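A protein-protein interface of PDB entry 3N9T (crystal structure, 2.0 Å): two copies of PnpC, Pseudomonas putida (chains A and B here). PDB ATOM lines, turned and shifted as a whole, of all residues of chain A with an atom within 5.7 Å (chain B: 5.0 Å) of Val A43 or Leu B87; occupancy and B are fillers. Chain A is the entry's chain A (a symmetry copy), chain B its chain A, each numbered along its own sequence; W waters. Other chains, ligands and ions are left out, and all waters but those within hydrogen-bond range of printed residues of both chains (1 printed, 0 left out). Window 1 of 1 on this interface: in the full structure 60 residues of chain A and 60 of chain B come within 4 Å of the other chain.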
ATOM      1  N   GLU A   9       7.454 -30.131  10.178  1.00  0.00           N
ATOM      2  CA  GLU A   9       8.287 -30.477  11.360  1.00  0.00           C
ATOM      3  C   GLU A   9       8.202 -31.957  11.670  1.00  0.00           C
ATOM      4  O   GLU A   9       9.226 -32.609  11.935  1.00  0.00           O
ATOM      5  CB  GLU A   9       7.899 -29.602  12.548  1.00  0.00           C
ATOM      6  CG  GLU A   9       8.244 -28.132  12.274  1.00  0.00           C
ATOM      7  CD  GLU A   9       7.505 -27.141  13.136  1.00  0.00           C
ATOM      8  OE1 GLU A   9       6.955 -27.535  14.223  1.00  0.00           O
ATOM      9  OE2 GLU A   9       7.520 -25.925  12.789  1.00  0.00           O
ATOM     10  N   ILE A  12      10.421 -33.963   9.267  1.00  0.00           N
ATOM     11  CA  ILE A  12      11.864 -33.927   9.569  1.00  0.00           C
ATOM     12  C   ILE A  12      12.161 -34.972  10.692  1.00  0.00           C
ATOM     13  O   ILE A  12      13.130 -35.742  10.651  1.00  0.00           O
ATOM     14  CB  ILE A  12      12.259 -32.482  10.052  1.00  0.00           C
ATOM     15  CG1 ILE A  12      12.112 -31.452   8.906  1.00  0.00           C
ATOM     16  CG2 ILE A  12      13.744 -32.492  10.715  1.00  0.00           C
ATOM     17  CD1 ILE A  12      12.132 -29.902   9.434  1.00  0.00           C
ATOM     18  N   SER A  13      11.336 -34.979  11.735  1.00  0.00           N
ATOM     19  CA  SER A  13      11.560 -35.962  12.829  1.00  0.00           C
ATOM     20  C   SER A  13      11.386 -37.411  12.407  1.00  0.00           C
ATOM     21  O   SER A  13      12.161 -38.291  12.833  1.00  0.00           O
ATOM     22  CB  SER A  13      10.656 -35.634  14.032  1.00  0.00           C
ATOM     23  OG  SER A  13      10.918 -34.277  14.361  1.00  0.00           O
ATOM     24  N   HIS A  38      12.851 -38.654  21.429  1.00  0.00           N
ATOM     25  CA  HIS A  38      12.766 -37.862  22.691  1.00  0.00           C
ATOM     26  C   HIS A  38      13.411 -36.500  22.504  1.00  0.00           C
ATOM     27  O   HIS A  38      12.882 -35.472  22.985  1.00  0.00           O
ATOM     28  CB  HIS A  38      13.342 -38.572  23.945  1.00  0.00           C
ATOM     29  CG  HIS A  38      12.511 -39.712  24.420  1.00  0.00           C
ATOM     30  ND1 HIS A  38      11.508 -39.567  25.355  1.00  0.00           N
ATOM     31  CD2 HIS A  38      12.423 -40.984  23.978  1.00  0.00           C
ATOM     32  CE1 HIS A  38      10.924 -40.742  25.565  1.00  0.00           C
ATOM     33  NE2 HIS A  38      11.429 -41.607  24.728  1.00  0.00           N
ATOM     34  N   LEU A  39      14.520 -36.489  21.798  1.00  0.00           N
ATOM     35  CA  LEU A  39      15.239 -35.246  21.583  1.00  0.00           C
ATOM     36  C   LEU A  39      14.377 -34.266  20.764  1.00  0.00           C
ATOM     37  O   LEU A  39      14.242 -33.080  21.112  1.00  0.00           O
ATOM     38  CB  LEU A  39      16.456 -35.602  20.757  1.00  0.00           C
ATOM     39  CG  LEU A  39      17.557 -34.601  20.476  1.00  0.00           C
ATOM     40  CD1 LEU A  39      17.916 -33.760  21.681  1.00  0.00           C
ATOM     41  CD2 LEU A  39      18.774 -35.426  19.943  1.00  0.00           C
ATOM     42  N   HIS A  40      13.778 -34.784  19.681  1.00  0.00           N
ATOM     43  CA  HIS A  40      12.928 -33.986  18.827  1.00  0.00           C
ATOM     44  C   HIS A  40      11.620 -33.590  19.541  1.00  0.00           C
ATOM     45  O   HIS A  40      11.180 -32.474  19.353  1.00  0.00           O
ATOM     46  CB  HIS A  40      12.550 -34.722  17.517  1.00  0.00           C
ATOM     47  CG  HIS A  40      13.643 -34.707  16.488  1.00  0.00           C
ATOM     48  ND1 HIS A  40      13.432 -34.273  15.193  1.00  0.00           N
ATOM     49  CD2 HIS A  40      14.960 -35.015  16.570  1.00  0.00           C
ATOM     50  CE1 HIS A  40      14.562 -34.371  14.511  1.00  0.00           C
ATOM     51  NE2 HIS A  40      15.501 -34.814  15.327  1.00  0.00           N
ATOM     52  N   ASP A  41      11.050 -34.476  20.368  1.00  0.00           N
ATOM     53  CA  ASP A  41       9.863 -34.090  21.148  1.00  0.00           C
ATOM     54  C   ASP A  41      10.180 -32.972  22.160  1.00  0.00           C
ATOM     55  O   ASP A  41       9.379 -32.076  22.400  1.00  0.00           O
ATOM     56  CB  ASP A  41       9.267 -35.284  21.872  1.00  0.00           C
ATOM     57  CG  ASP A  41       8.433 -36.200  20.916  1.00  0.00           C
ATOM     58  OD1 ASP A  41       8.146 -35.805  19.760  1.00  0.00           O
ATOM     59  OD2 ASP A  41       8.090 -37.307  21.355  1.00  0.00           O
ATOM     60  N   PHE A  42      11.328 -33.066  22.796  1.00  0.00           N
ATOM     61  CA  PHE A  42      11.790 -31.971  23.634  1.00  0.00           C
ATOM     62  C   PHE A  42      11.902 -30.617  22.891  1.00  0.00           C
ATOM     63  O   PHE A  42      11.370 -29.548  23.346  1.00  0.00           O
ATOM     64  CB  PHE A  42      13.126 -32.371  24.268  1.00  0.00           C
ATOM     65  CG  PHE A  42      13.958 -31.200  24.675  1.00  0.00           C
ATOM     66  CD1 PHE A  42      13.534 -30.352  25.738  1.00  0.00           C
ATOM     67  CD2 PHE A  42      15.162 -30.942  24.037  1.00  0.00           C
ATOM     68  CE1 PHE A  42      14.309 -29.275  26.103  1.00  0.00           C
ATOM     69  CE2 PHE A  42      15.906 -29.836  24.377  1.00  0.00           C
ATOM     70  CZ  PHE A  42      15.496 -29.026  25.441  1.00  0.00           C
ATOM     71  N   VAL A  43      12.629 -30.630  21.790  1.00  0.00           N
ATOM     72  CA  VAL A  43      12.827 -29.392  21.011  1.00  0.00           C
ATOM     73  C   VAL A  43      11.437 -28.815  20.569  1.00  0.00           C
ATOM     74  O   VAL A  43      11.194 -27.624  20.641  1.00  0.00           O
ATOM     75  CB  VAL A  43      13.713 -29.675  19.809  1.00  0.00           C
ATOM     76  CG1 VAL A  43      13.727 -28.505  18.824  1.00  0.00           C
ATOM     77  CG2 VAL A  43      15.157 -29.946  20.264  1.00  0.00           C
ATOM     78  N   SER A  44      10.563 -29.679  20.116  1.00  0.00           N
ATOM     79  CA  SER A  44       9.207 -29.285  19.688  1.00  0.00           C
ATOM     80  C   SER A  44       8.358 -28.756  20.840  1.00  0.00           C
ATOM     81  O   SER A  44       7.636 -27.773  20.656  1.00  0.00           O
ATOM     82  CB  SER A  44       8.502 -30.500  19.111  1.00  0.00           C
ATOM     83  OG  SER A  44       9.027 -30.662  17.831  1.00  0.00           O
ATOM     84  N   GLU A  45       8.384 -29.471  21.988  1.00  0.00           N
ATOM     85  CA  GLU A  45       7.630 -29.081  23.186  1.00  0.00           C
ATOM     86  C   GLU A  45       7.932 -27.655  23.613  1.00  0.00           C
ATOM     87  O   GLU A  45       7.025 -26.843  23.867  1.00  0.00           O
ATOM     88  CB  GLU A  45       7.957 -30.005  24.391  1.00  0.00           C
ATOM     89  CG  GLU A  45       7.146 -29.610  25.628  1.00  0.00           C
ATOM     90  CD  GLU A  45       7.109 -30.680  26.696  1.00  0.00           C
ATOM     91  OE1 GLU A  45       8.064 -30.835  27.453  1.00  0.00           O
ATOM     92  OE2 GLU A  45       6.092 -31.377  26.773  1.00  0.00           O
ATOM     93  N   VAL A  46       9.209 -27.350  23.749  1.00  0.00           N
ATOM     94  CA  VAL A  46       9.600 -26.053  24.256  1.00  0.00           C
ATOM     95  C   VAL A  46       9.741 -24.969  23.144  1.00  0.00           C
ATOM     96  O   VAL A  46       9.926 -23.782  23.465  1.00  0.00           O
ATOM     97  CB  VAL A  46      10.953 -26.089  25.136  1.00  0.00           C
ATOM     98  CG1 VAL A  46      10.813 -27.037  26.327  1.00  0.00           C
ATOM     99  CG2 VAL A  46      12.193 -26.428  24.255  1.00  0.00           C
ATOM    100  N   GLU A  47       9.750 -25.413  21.876  1.00  0.00           N
ATOM    101  CA  GLU A  47       9.947 -24.531  20.695  1.00  0.00           C
ATOM    102  C   GLU A  47      11.254 -23.819  20.830  1.00  0.00           C
ATOM    103  O   GLU A  47      11.330 -22.591  20.881  1.00  0.00           O
ATOM    104  CB  GLU A  47       8.730 -23.606  20.527  1.00  0.00           C
ATOM    105  CG  GLU A  47       7.514 -24.495  20.261  1.00  0.00           C
ATOM    106  CD  GLU A  47       6.273 -23.755  19.791  1.00  0.00           C
ATOM    107  OE1 GLU A  47       6.118 -22.591  20.113  1.00  0.00           O
ATOM    108  OE2 GLU A  47       5.457 -24.361  19.100  1.00  0.00           O
ATOM    109  N   LEU A  48      12.314 -24.618  20.991  1.00  0.00           N
ATOM    110  CA  LEU A  48      13.656 -24.102  21.185  1.00  0.00           C
ATOM    111  C   LEU A  48      14.033 -23.046  20.122  1.00  0.00           C
ATOM    112  O   LEU A  48      13.814 -23.271  18.906  1.00  0.00           O
ATOM    113  CB  LEU A  48      14.670 -25.302  21.084  1.00  0.00           C
ATOM    114  CG  LEU A  48      16.011 -25.130  21.802  1.00  0.00           C
ATOM    115  CD1 LEU A  48      15.735 -25.202  23.303  1.00  0.00           C
ATOM    116  CD2 LEU A  48      16.947 -26.284  21.416  1.00  0.00           C
ATOM    117  N   GLY B  83      19.138 -34.587  13.010  1.00  0.00           N
ATOM    118  CA  GLY B  83      17.946 -33.831  12.504  1.00  0.00           C
ATOM    119  C   GLY B  83      17.483 -32.675  13.396  1.00  0.00           C
ATOM    120  O   GLY B  83      16.454 -32.013  13.128  1.00  0.00           O
ATOM    121  N   VAL B  84      18.260 -32.416  14.432  1.00  0.00           N
ATOM    122  CA  VAL B  84      17.905 -31.371  15.366  1.00  0.00           C
ATOM    123  C   VAL B  84      18.081 -29.979  14.718  1.00  0.00           C
ATOM    124  O   VAL B  84      17.234 -29.129  14.890  1.00  0.00           O
ATOM    125  CB  VAL B  84      18.717 -31.481  16.664  1.00  0.00           C
ATOM    126  CG1 VAL B  84      18.409 -30.276  17.556  1.00  0.00           C
ATOM    127  CG2 VAL B  84      18.288 -32.748  17.420  1.00  0.00           C
ATOM    128  N   SER B  85      19.102 -29.791  13.910  1.00  0.00           N
ATOM    129  CA  SER B  85      19.337 -28.455  13.358  1.00  0.00           C
ATOM    130  C   SER B  85      18.189 -28.083  12.417  1.00  0.00           C
ATOM    131  O   SER B  85      17.725 -26.956  12.436  1.00  0.00           O
ATOM    132  CB  SER B  85      20.663 -28.428  12.622  1.00  0.00           C
ATOM    133  OG  SER B  85      21.642 -28.983  13.483  1.00  0.00           O
ATOM    134  N   MET B  86      17.778 -29.016  11.560  1.00  0.00           N
ATOM    135  CA  MET B  86      16.660 -28.737  10.616  1.00  0.00           C
ATOM    136  C   MET B  86      15.317 -28.545  11.334  1.00  0.00           C
ATOM    137  O   MET B  86      14.489 -27.683  10.940  1.00  0.00           O
ATOM    138  CB  MET B  86      16.590 -29.809   9.523  1.00  0.00           C
ATOM    139  CG  MET B  86      17.743 -29.552   8.386  1.00  0.00           C
ATOM    140  SD  MET B  86      17.447 -28.045   7.377  1.00  0.00           S
ATOM    141  CE  MET B  86      15.732 -28.432   6.863  1.00  0.00           C
ATOM    142  N   LEU B  87      15.107 -29.333  12.409  1.00  0.00           N
ATOM    143  CA  LEU B  87      13.902 -29.163  13.244  1.00  0.00           C
ATOM    144  C   LEU B  87      13.868 -27.761  13.835  1.00  0.00           C
ATOM    145  O   LEU B  87      12.831 -27.062  13.750  1.00  0.00           O
ATOM    146  CB  LEU B  87      13.798 -30.230  14.347  1.00  0.00           C
ATOM    147  CG  LEU B  87      12.594 -30.033  15.283  1.00  0.00           C
ATOM    148  CD1 LEU B  87      11.332 -30.193  14.496  1.00  0.00           C
ATOM    149  CD2 LEU B  87      12.580 -31.066  16.356  1.00  0.00           C
ATOM    150  N   VAL B  88      15.005 -27.317  14.394  1.00  0.00           N
ATOM    151  CA  VAL B  88      15.089 -25.988  15.012  1.00  0.00           C
ATOM    152  C   VAL B  88      14.816 -24.880  13.949  1.00  0.00           C
ATOM    153  O   VAL B  88      14.073 -23.888  14.189  1.00  0.00           O
ATOM    154  CB  VAL B  88      16.466 -25.801  15.764  1.00  0.00           C
ATOM    155  CG1 VAL B  88      16.793 -24.336  16.098  1.00  0.00           C
ATOM    156  CG2 VAL B  88      16.474 -26.674  17.080  1.00  0.00           C
ATOM    157  N   ASP B  89      15.410 -25.062  12.768  1.00  0.00           N
ATOM    158  CA  ASP B  89      15.247 -24.054  11.721  1.00  0.00           C
ATOM    159  C   ASP B  89      13.738 -23.974  11.350  1.00  0.00           C
ATOM    160  O   ASP B  89      13.181 -22.887  11.186  1.00  0.00           O
ATOM    161  CB  ASP B  89      16.008 -24.491  10.455  1.00  0.00           C
ATOM    162  CG  ASP B  89      15.675 -23.549   9.273  1.00  0.00           C
ATOM    163  OD1 ASP B  89      16.064 -22.371   9.382  1.00  0.00           O
ATOM    164  OD2 ASP B  89      14.994 -23.967   8.328  1.00  0.00           O
ATOM    165  N   ALA B  90      13.062 -25.126  11.245  1.00  0.00           N
ATOM    166  CA  ALA B  90      11.622 -25.085  10.837  1.00  0.00           C
ATOM    167  C   ALA B  90      10.779 -24.396  11.883  1.00  0.00           C
ATOM    168  O   ALA B  90       9.929 -23.531  11.567  1.00  0.00           O
ATOM    169  CB  ALA B  90      11.077 -26.571  10.578  1.00  0.00           C
ATOM    170  N   ILE B  91      11.047 -24.734  13.149  1.00  0.00           N
ATOM    171  CA  ILE B  91      10.256 -24.184  14.275  1.00  0.00           C
ATOM    172  C   ILE B  91      10.329 -22.680  14.328  1.00  0.00           C
ATOM    173  O   ILE B  91       9.354 -22.030  14.660  1.00  0.00           O
ATOM    174  CB  ILE B  91      10.697 -24.755  15.627  1.00  0.00           C
ATOM    175  CG1 ILE B  91      10.368 -26.243  15.670  1.00  0.00           C
ATOM    176  CG2 ILE B  91      10.149 -23.935  16.841  1.00  0.00           C
ATOM    177  CD1 ILE B  91      10.929 -26.894  16.970  1.00  0.00           C
HETATM  178  O   HOH W   1       7.707 -25.302  10.267  1.00  0.00           O
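The backbone carbonyl oxygen (O) of Glu A9 sits at hydrogen-bond distance from the side-chain hydroxyl (OG) of Ser A13 (3.4 Å).
The side-chain hydroxyl of Ser A13 is in hydrogen-bond range of a ring nitrogen (ND1) of His A40 (2.6 Å).
The backbone carbonyl oxygen (O) of His A40 sits at hydrogen-bond distance from the side-chain hydroxyl (OG) of Ser A44 (3.2 Å).
The backbone NH (N) of Leu A48 lies within hydrogen-bond range of the backbone carbonyl oxygen (O) of Val A43.
CA of Ile B91 touches OE2 of Glu A9, 3.6 Å away.
CG2 of Ile A12 touches O of Gly B83 (3.7 Å).
Met B86 touches Ile A12.
Ile A12 touches Leu B87.
Ile A12 touches Ala B90 (CD1 to CB, 3.7 Å).
His A40 touches Gly B83.
Val B84 touches His A40 (N to NE2, 3.8 Å).
His A40 touches Leu B87 (ND1 to CD2, 3.5 Å).
Leu B87 touches Val A43.
Leu B87 touches Ser A44.
Of chain B, only Leu B87 (3.7 Å), Val B88 (3.7 Å) and Ile B91 (3.7 Å) come within 4 Å of Val A43.
Of the printed residues of chain A, Met B86 touches Ile A12.
Of the printed residues of chain B, Glu A9 touches Leu B87 (3.99 Å), Ala B90 (3.6 Å) and Ile B91 (3.6 Å).
Printed residues of chain B within 4 Å of Ile A12: Gly B83, Met B86, Leu B87 and Ala B90.
Printed residues of chain B within 4 Å of His A40: Gly B83, Val B84 and Leu B87.
Of the printed residues of chain B, Ser A44 touches Leu B87 (3.9 Å).
Asp A41 touches none of the printed residues of chain B.
Ser B85 touches none of the printed residues of chain A.
The nearest residue of chain B that does not touch Val A43 is Val B84 (4.2 Å).
Of the 9 printed residues of chain B, 7 touch a printed residue of chain A.
Hydrophobic or aromatic side chains of chain B that line the printed part of chain A: Val B84, Leu B87, Val B88, Ala B90 and Ile B91.
Hydrophobic or aromatic side chains of chain A that line the printed part of chain B: Ile A12, Leu A39, His A40 and Val A43.
Among the printed residues, no Asp or Glu carboxylate lies within 4 Å of a Lys or Arg side-chain nitrogen of the other chain.
No position is printed for both chains.
Water W1 bridges the side-chain carboxylate of Glu A9 and the backbone carbonyl oxygen of Ala B90.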
